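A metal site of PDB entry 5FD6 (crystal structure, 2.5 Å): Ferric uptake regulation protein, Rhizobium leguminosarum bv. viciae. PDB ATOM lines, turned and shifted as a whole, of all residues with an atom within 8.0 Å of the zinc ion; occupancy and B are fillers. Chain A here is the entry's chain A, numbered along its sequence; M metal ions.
The guanidinium group (NE) of Arg 82 lies within hydrogen-bond range of the backbone carbonyl oxygen (O) of His 36.
ND1 of His 91 lies close to OE1 of Glu 104 (3.4 Å).
The side-chain carboxylate (OE1) of Glu 84 sits at hydrogen-bond distance from a ring nitrogen (NE2) of His 36, 3.3 Å away.
The backbone NH (N) of Ala 72 lies within hydrogen-bond range of the backbone carbonyl oxygen (O) of Glu 84.
Merely in contact with the zinc ion: His 36.
Of the 22 residues printed, 4 come within 4 Å of the zinc ion.
The zinc ion is bound by OE2 of Glu 84, NE2 of His 93 and NE2 of His 91.
The zinc ion has three donor atoms within binding distance.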
ATOM      1  N   GLU A  34      -8.572 -34.144 -31.219  1.00  0.00           N
ATOM      2  CA  GLU A  34      -8.983 -32.921 -30.535  1.00  0.00           C
ATOM      3  C   GLU A  34      -9.452 -33.177 -29.095  1.00  0.00           C
ATOM      4  O   GLU A  34      -9.552 -32.229 -28.317  1.00  0.00           O
ATOM      5  CB  GLU A  34     -10.096 -32.235 -31.328  1.00  0.00           C
ATOM      6  CG  GLU A  34      -9.599 -31.618 -32.624  1.00  0.00           C
ATOM      7  CD  GLU A  34     -10.569 -30.641 -33.250  1.00  0.00           C
ATOM      8  OE1 GLU A  34     -11.423 -30.074 -32.524  1.00  0.00           O
ATOM      9  OE2 GLU A  34     -10.461 -30.423 -34.476  1.00  0.00           O
ATOM     10  N   ASP A  35      -9.816 -34.414 -28.772  1.00  0.00           N
ATOM     11  CA  ASP A  35      -9.920 -34.865 -27.406  1.00  0.00           C
ATOM     12  C   ASP A  35      -8.468 -35.108 -27.051  1.00  0.00           C
ATOM     13  O   ASP A  35      -7.730 -35.604 -27.878  1.00  0.00           O
ATOM     14  CB  ASP A  35     -10.814 -36.137 -27.290  1.00  0.00           C
ATOM     15  CG  ASP A  35     -10.099 -37.406 -27.759  1.00  0.00           C
ATOM     16  OD1 ASP A  35      -9.577 -37.413 -28.888  1.00  0.00           O
ATOM     17  OD2 ASP A  35     -10.052 -38.402 -27.017  1.00  0.00           O
ATOM     18  N   HIS A  36      -8.028 -34.690 -25.879  1.00  0.00           N
ATOM     19  CA  HIS A  36      -6.588 -34.621 -25.608  1.00  0.00           C
ATOM     20  C   HIS A  36      -6.182 -35.963 -24.994  1.00  0.00           C
ATOM     21  O   HIS A  36      -6.163 -36.098 -23.774  1.00  0.00           O
ATOM     22  CB  HIS A  36      -6.260 -33.445 -24.676  1.00  0.00           C
ATOM     23  CG  HIS A  36      -6.658 -32.104 -25.231  1.00  0.00           C
ATOM     24  ND1 HIS A  36      -7.431 -31.218 -24.527  1.00  0.00           N
ATOM     25  CD2 HIS A  36      -6.421 -31.524 -26.423  1.00  0.00           C
ATOM     26  CE1 HIS A  36      -7.634 -30.136 -25.255  1.00  0.00           C
ATOM     27  NE2 HIS A  36      -7.023 -30.295 -26.408  1.00  0.00           N
ATOM     28  N   ALA A  72       2.058 -30.539 -25.374  1.00  0.00           N
ATOM     29  CA  ALA A  72       1.714 -29.976 -24.082  1.00  0.00           C
ATOM     30  C   ALA A  72       1.001 -31.056 -23.233  1.00  0.00           C
ATOM     31  O   ALA A  72      -0.011 -31.594 -23.644  1.00  0.00           O
ATOM     32  CB  ALA A  72       0.780 -28.794 -24.277  1.00  0.00           C
ATOM     33  N   HIS A  74      -1.188 -31.917 -19.875  1.00  0.00           N
ATOM     34  CA  HIS A  74      -2.141 -31.283 -18.958  1.00  0.00           C
ATOM     35  C   HIS A  74      -2.595 -32.263 -17.895  1.00  0.00           C
ATOM     36  O   HIS A  74      -3.120 -33.320 -18.217  1.00  0.00           O
ATOM     37  CB  HIS A  74      -3.354 -30.768 -19.717  1.00  0.00           C
ATOM     38  CG  HIS A  74      -3.103 -29.473 -20.423  1.00  0.00           C
ATOM     39  ND1 HIS A  74      -3.109 -28.262 -19.763  1.00  0.00           N
ATOM     40  CD2 HIS A  74      -2.837 -29.209 -21.720  1.00  0.00           C
ATOM     41  CE1 HIS A  74      -2.845 -27.304 -20.636  1.00  0.00           C
ATOM     42  NE2 HIS A  74      -2.670 -27.855 -21.816  1.00  0.00           N
ATOM     43  N   PHE A  76      -5.309 -32.388 -15.512  1.00  0.00           N
ATOM     44  CA  PHE A  76      -6.592 -31.978 -15.000  1.00  0.00           C
ATOM     45  C   PHE A  76      -6.961 -32.901 -13.842  1.00  0.00           C
ATOM     46  O   PHE A  76      -6.511 -34.055 -13.797  1.00  0.00           O
ATOM     47  CB  PHE A  76      -7.602 -32.028 -16.143  1.00  0.00           C
ATOM     48  CG  PHE A  76      -7.261 -31.097 -17.290  1.00  0.00           C
ATOM     49  CD1 PHE A  76      -7.183 -29.718 -17.084  1.00  0.00           C
ATOM     50  CD2 PHE A  76      -7.027 -31.580 -18.570  1.00  0.00           C
ATOM     51  CE1 PHE A  76      -6.891 -28.864 -18.127  1.00  0.00           C
ATOM     52  CE2 PHE A  76      -6.726 -30.725 -19.609  1.00  0.00           C
ATOM     53  CZ  PHE A  76      -6.650 -29.366 -19.395  1.00  0.00           C
ATOM     54  N   ARG A  82      -3.435 -35.505 -19.816  1.00  0.00           N
ATOM     55  CA  ARG A  82      -3.939 -35.312 -21.163  1.00  0.00           C
ATOM     56  C   ARG A  82      -2.888 -34.603 -21.988  1.00  0.00           C
ATOM     57  O   ARG A  82      -2.212 -33.706 -21.502  1.00  0.00           O
ATOM     58  CB  ARG A  82      -5.191 -34.436 -21.143  1.00  0.00           C
ATOM     59  CG  ARG A  82      -6.256 -34.779 -20.105  1.00  0.00           C
ATOM     60  CD  ARG A  82      -6.879 -36.140 -20.292  1.00  0.00           C
ATOM     61  NE  ARG A  82      -7.569 -36.277 -21.576  1.00  0.00           N
ATOM     62  CZ  ARG A  82      -8.327 -37.316 -21.920  1.00  0.00           C
ATOM     63  NH1 ARG A  82      -8.500 -38.305 -21.075  1.00  0.00           N
ATOM     64  NH2 ARG A  82      -8.906 -37.384 -23.120  1.00  0.00           N
ATOM     65  N   TYR A  83      -2.768 -35.006 -23.247  1.00  0.00           N
ATOM     66  CA  TYR A  83      -1.716 -34.517 -24.107  1.00  0.00           C
ATOM     67  C   TYR A  83      -2.292 -33.961 -25.386  1.00  0.00           C
ATOM     68  O   TYR A  83      -3.275 -34.484 -25.915  1.00  0.00           O
ATOM     69  CB  TYR A  83      -0.757 -35.646 -24.410  1.00  0.00           C
ATOM     70  CG  TYR A  83       0.041 -36.139 -23.228  1.00  0.00           C
ATOM     71  CD1 TYR A  83       1.290 -35.616 -22.934  1.00  0.00           C
ATOM     72  CD2 TYR A  83      -0.455 -37.158 -22.413  1.00  0.00           C
ATOM     73  CE1 TYR A  83       2.034 -36.082 -21.860  1.00  0.00           C
ATOM     74  CE2 TYR A  83       0.290 -37.634 -21.340  1.00  0.00           C
ATOM     75  CZ  TYR A  83       1.523 -37.092 -21.062  1.00  0.00           C
ATOM     76  OH  TYR A  83       2.261 -37.548 -20.002  1.00  0.00           O
ATOM     77  N   GLU A  84      -1.666 -32.906 -25.903  1.00  0.00           N
ATOM     78  CA  GLU A  84      -2.029 -32.380 -27.213  1.00  0.00           C
ATOM     79  C   GLU A  84      -0.859 -31.772 -27.939  1.00  0.00           C
ATOM     80  O   GLU A  84       0.159 -31.418 -27.330  1.00  0.00           O
ATOM     81  CB  GLU A  84      -3.120 -31.320 -27.069  1.00  0.00           C
ATOM     82  CG  GLU A  84      -2.700 -30.103 -26.259  1.00  0.00           C
ATOM     83  CD  GLU A  84      -3.732 -28.994 -26.261  1.00  0.00           C
ATOM     84  OE1 GLU A  84      -4.300 -28.683 -27.334  1.00  0.00           O
ATOM     85  OE2 GLU A  84      -3.970 -28.397 -25.172  1.00  0.00           O
ATOM     86  N   THR A  85      -1.039 -31.610 -29.248  1.00  0.00           N
ATOM     87  CA  THR A  85      -0.082 -30.909 -30.081  1.00  0.00           C
ATOM     88  C   THR A  85      -0.155 -29.480 -29.610  1.00  0.00           C
ATOM     89  O   THR A  85      -1.259 -28.986 -29.354  1.00  0.00           O
ATOM     90  CB  THR A  85      -0.405 -30.967 -31.595  1.00  0.00           C
ATOM     91  OG1 THR A  85      -1.625 -30.251 -31.898  1.00  0.00           O
ATOM     92  CG2 THR A  85      -0.511 -32.404 -32.055  1.00  0.00           C
ATOM     93  N   VAL A  86       0.994 -28.833 -29.438  1.00  0.00           N
ATOM     94  CA  VAL A  86       1.028 -27.443 -28.978  1.00  0.00           C
ATOM     95  C   VAL A  86       0.016 -26.607 -29.784  1.00  0.00           C
ATOM     96  O   VAL A  86       0.072 -26.595 -31.001  1.00  0.00           O
ATOM     97  CB  VAL A  86       2.443 -26.818 -28.988  1.00  0.00           C
ATOM     98  CG1 VAL A  86       3.167 -26.992 -30.323  1.00  0.00           C
ATOM     99  CG2 VAL A  86       2.392 -25.344 -28.603  1.00  0.00           C
ATOM    100  N   PRO A  87      -0.952 -25.949 -29.090  1.00  0.00           N
ATOM    101  CA  PRO A  87      -1.984 -25.237 -29.824  1.00  0.00           C
ATOM    102  C   PRO A  87      -1.458 -23.929 -30.412  1.00  0.00           C
ATOM    103  O   PRO A  87      -0.745 -23.173 -29.733  1.00  0.00           O
ATOM    104  CB  PRO A  87      -3.078 -24.990 -28.784  1.00  0.00           C
ATOM    105  CG  PRO A  87      -2.466 -25.233 -27.448  1.00  0.00           C
ATOM    106  CD  PRO A  87      -1.095 -25.793 -27.627  1.00  0.00           C
ATOM    107  N   GLU A  89      -3.191 -21.370 -31.278  1.00  0.00           N
ATOM    108  CA  GLU A  89      -3.814 -20.310 -30.498  1.00  0.00           C
ATOM    109  C   GLU A  89      -4.291 -20.846 -29.166  1.00  0.00           C
ATOM    110  O   GLU A  89      -4.705 -21.993 -29.044  1.00  0.00           O
ATOM    111  CB  GLU A  89      -4.969 -19.639 -31.244  1.00  0.00           C
ATOM    112  CG  GLU A  89      -6.025 -20.591 -31.776  1.00  0.00           C
ATOM    113  CD  GLU A  89      -7.217 -19.876 -32.394  1.00  0.00           C
ATOM    114  OE1 GLU A  89      -7.099 -18.682 -32.749  1.00  0.00           O
ATOM    115  OE2 GLU A  89      -8.275 -20.515 -32.526  1.00  0.00           O
ATOM    116  N   HIS A  90      -4.223 -19.977 -28.180  1.00  0.00           N
ATOM    117  CA  HIS A  90      -4.709 -20.263 -26.848  1.00  0.00           C
ATOM    118  C   HIS A  90      -6.188 -20.662 -26.862  1.00  0.00           C
ATOM    119  O   HIS A  90      -6.984 -20.138 -27.627  1.00  0.00           O
ATOM    120  CB  HIS A  90      -4.504 -19.016 -25.975  1.00  0.00           C
ATOM    121  CG  HIS A  90      -5.511 -18.893 -24.884  1.00  0.00           C
ATOM    122  ND1 HIS A  90      -5.378 -19.510 -23.656  1.00  0.00           N
ATOM    123  CD2 HIS A  90      -6.705 -18.243 -24.853  1.00  0.00           C
ATOM    124  CE1 HIS A  90      -6.434 -19.224 -22.913  1.00  0.00           C
ATOM    125  NE2 HIS A  90      -7.244 -18.461 -23.615  1.00  0.00           N
ATOM    126  N   HIS A  91      -6.526 -21.597 -25.975  1.00  0.00           N
ATOM    127  CA  HIS A  91      -7.910 -21.945 -25.662  1.00  0.00           C
ATOM    128  C   HIS A  91      -7.985 -22.476 -24.223  1.00  0.00           C
ATOM    129  O   HIS A  91      -6.969 -22.875 -23.640  1.00  0.00           O
ATOM    130  CB  HIS A  91      -8.440 -23.009 -26.629  1.00  0.00           C
ATOM    131  CG  HIS A  91      -7.716 -24.319 -26.531  1.00  0.00           C
ATOM    132  ND1 HIS A  91      -6.904 -24.794 -27.532  1.00  0.00           N
ATOM    133  CD2 HIS A  91      -7.627 -25.217 -25.525  1.00  0.00           C
ATOM    134  CE1 HIS A  91      -6.374 -25.938 -27.169  1.00  0.00           C
ATOM    135  NE2 HIS A  91      -6.800 -26.225 -25.953  1.00  0.00           N
ATOM    136  N   ASP A  92      -9.193 -22.520 -23.697  1.00  0.00           N
ATOM    137  CA  ASP A  92      -9.459 -23.086 -22.364  1.00  0.00           C
ATOM    138  C   ASP A  92     -10.025 -24.493 -22.475  1.00  0.00           C
ATOM    139  O   ASP A  92     -10.220 -25.000 -23.592  1.00  0.00           O
ATOM    140  CB  ASP A  92     -10.371 -22.114 -21.583  1.00  0.00           C
ATOM    141  CG  ASP A  92      -9.683 -20.789 -21.337  1.00  0.00           C
ATOM    142  OD1 ASP A  92      -8.485 -20.844 -21.014  1.00  0.00           O
ATOM    143  OD2 ASP A  92     -10.272 -19.705 -21.500  1.00  0.00           O
ATOM    144  N   HIS A  93     -10.255 -25.132 -21.338  1.00  0.00           N
ATOM    145  CA  HIS A  93     -10.631 -26.545 -21.303  1.00  0.00           C
ATOM    146  C   HIS A  93     -11.874 -26.850 -20.492  1.00  0.00           C
ATOM    147  O   HIS A  93     -12.070 -26.310 -19.387  1.00  0.00           O
ATOM    148  CB  HIS A  93      -9.475 -27.323 -20.716  1.00  0.00           C
ATOM    149  CG  HIS A  93      -8.263 -27.351 -21.593  1.00  0.00           C
ATOM    150  ND1 HIS A  93      -7.228 -26.463 -21.456  1.00  0.00           N
ATOM    151  CD2 HIS A  93      -7.937 -28.162 -22.615  1.00  0.00           C
ATOM    152  CE1 HIS A  93      -6.294 -26.737 -22.348  1.00  0.00           C
ATOM    153  NE2 HIS A  93      -6.696 -27.764 -23.062  1.00  0.00           N
ATOM    154  N   LEU A  94     -12.722 -27.691 -21.070  1.00  0.00           N
ATOM    155  CA  LEU A  94     -13.863 -28.315 -20.408  1.00  0.00           C
ATOM    156  C   LEU A  94     -13.606 -29.837 -20.425  1.00  0.00           C
ATOM    157  O   LEU A  94     -13.222 -30.381 -21.460  1.00  0.00           O
ATOM    158  CB  LEU A  94     -15.126 -27.994 -21.190  1.00  0.00           C
ATOM    159  CG  LEU A  94     -16.480 -28.651 -20.861  1.00  0.00           C
ATOM    160  CD1 LEU A  94     -16.978 -28.266 -19.482  1.00  0.00           C
ATOM    161  CD2 LEU A  94     -17.476 -28.229 -21.926  1.00  0.00           C
ATOM    162  N   VAL A 102     -11.620 -34.504 -23.144  1.00  0.00           N
ATOM    163  CA  VAL A 102     -11.511 -33.040 -23.050  1.00  0.00           C
ATOM    164  C   VAL A 102     -12.039 -32.289 -24.275  1.00  0.00           C
ATOM    165  O   VAL A 102     -11.781 -32.672 -25.430  1.00  0.00           O
ATOM    166  CB  VAL A 102     -10.047 -32.626 -22.802  1.00  0.00           C
ATOM    167  CG1 VAL A 102      -9.946 -31.114 -22.600  1.00  0.00           C
ATOM    168  CG2 VAL A 102      -9.500 -33.325 -21.555  1.00  0.00           C
ATOM    169  N   ILE A 103     -12.756 -31.207 -23.992  1.00  0.00           N
ATOM    170  CA  ILE A 103     -13.290 -30.302 -24.981  1.00  0.00           C
ATOM    171  C   ILE A 103     -12.605 -28.935 -24.811  1.00  0.00           C
ATOM    172  O   ILE A 103     -12.610 -28.376 -23.722  1.00  0.00           O
ATOM    173  CB  ILE A 103     -14.832 -30.159 -24.804  1.00  0.00           C
ATOM    174  CG1 ILE A 103     -15.516 -31.492 -25.135  1.00  0.00           C
ATOM    175  CG2 ILE A 103     -15.387 -28.998 -25.644  1.00  0.00           C
ATOM    176  CD1 ILE A 103     -15.559 -32.486 -23.983  1.00  0.00           C
ATOM    177  N   GLU A 104     -12.022 -28.435 -25.903  1.00  0.00           N
ATOM    178  CA  GLU A 104     -11.430 -27.082 -25.970  1.00  0.00           C
ATOM    179  C   GLU A 104     -12.477 -26.017 -26.308  1.00  0.00           C
ATOM    180  O   GLU A 104     -13.469 -26.297 -26.967  1.00  0.00           O
ATOM    181  CB  GLU A 104     -10.249 -27.039 -26.965  1.00  0.00           C
ATOM    182  CG  GLU A 104     -10.509 -27.515 -28.391  1.00  0.00           C
ATOM    183  CD  GLU A 104      -9.230 -27.962 -29.114  1.00  0.00           C
ATOM    184  OE1 GLU A 104      -8.425 -27.085 -29.478  1.00  0.00           O
ATOM    185  OE2 GLU A 104      -9.037 -29.175 -29.324  1.00  0.00           O
ATOM    186  N   PHE A 105     -12.256 -24.791 -25.822  1.00  0.00           N
ATOM    187  CA  PHE A 105     -13.119 -23.661 -26.120  1.00  0.00           C
ATOM    188  C   PHE A 105     -12.391 -22.330 -25.967  1.00  0.00           C
ATOM    189  O   PHE A 105     -11.475 -22.201 -25.153  1.00  0.00           O
ATOM    190  CB  PHE A 105     -14.415 -23.680 -25.292  1.00  0.00           C
ATOM    191  CG  PHE A 105     -14.226 -23.453 -23.803  1.00  0.00           C
ATOM    192  CD1 PHE A 105     -14.250 -22.171 -23.266  1.00  0.00           C
ATOM    193  CD2 PHE A 105     -14.083 -24.533 -22.938  1.00  0.00           C
ATOM    194  CE1 PHE A 105     -14.106 -21.966 -21.896  1.00  0.00           C
ATOM    195  CE2 PHE A 105     -13.935 -24.328 -21.576  1.00  0.00           C
ATOM    196  CZ  PHE A 105     -13.964 -23.056 -21.052  1.00  0.00           C
HETATM  197 ZN    ZN M   1      -5.892 -27.958 -25.007  1.00  0.00          ZN
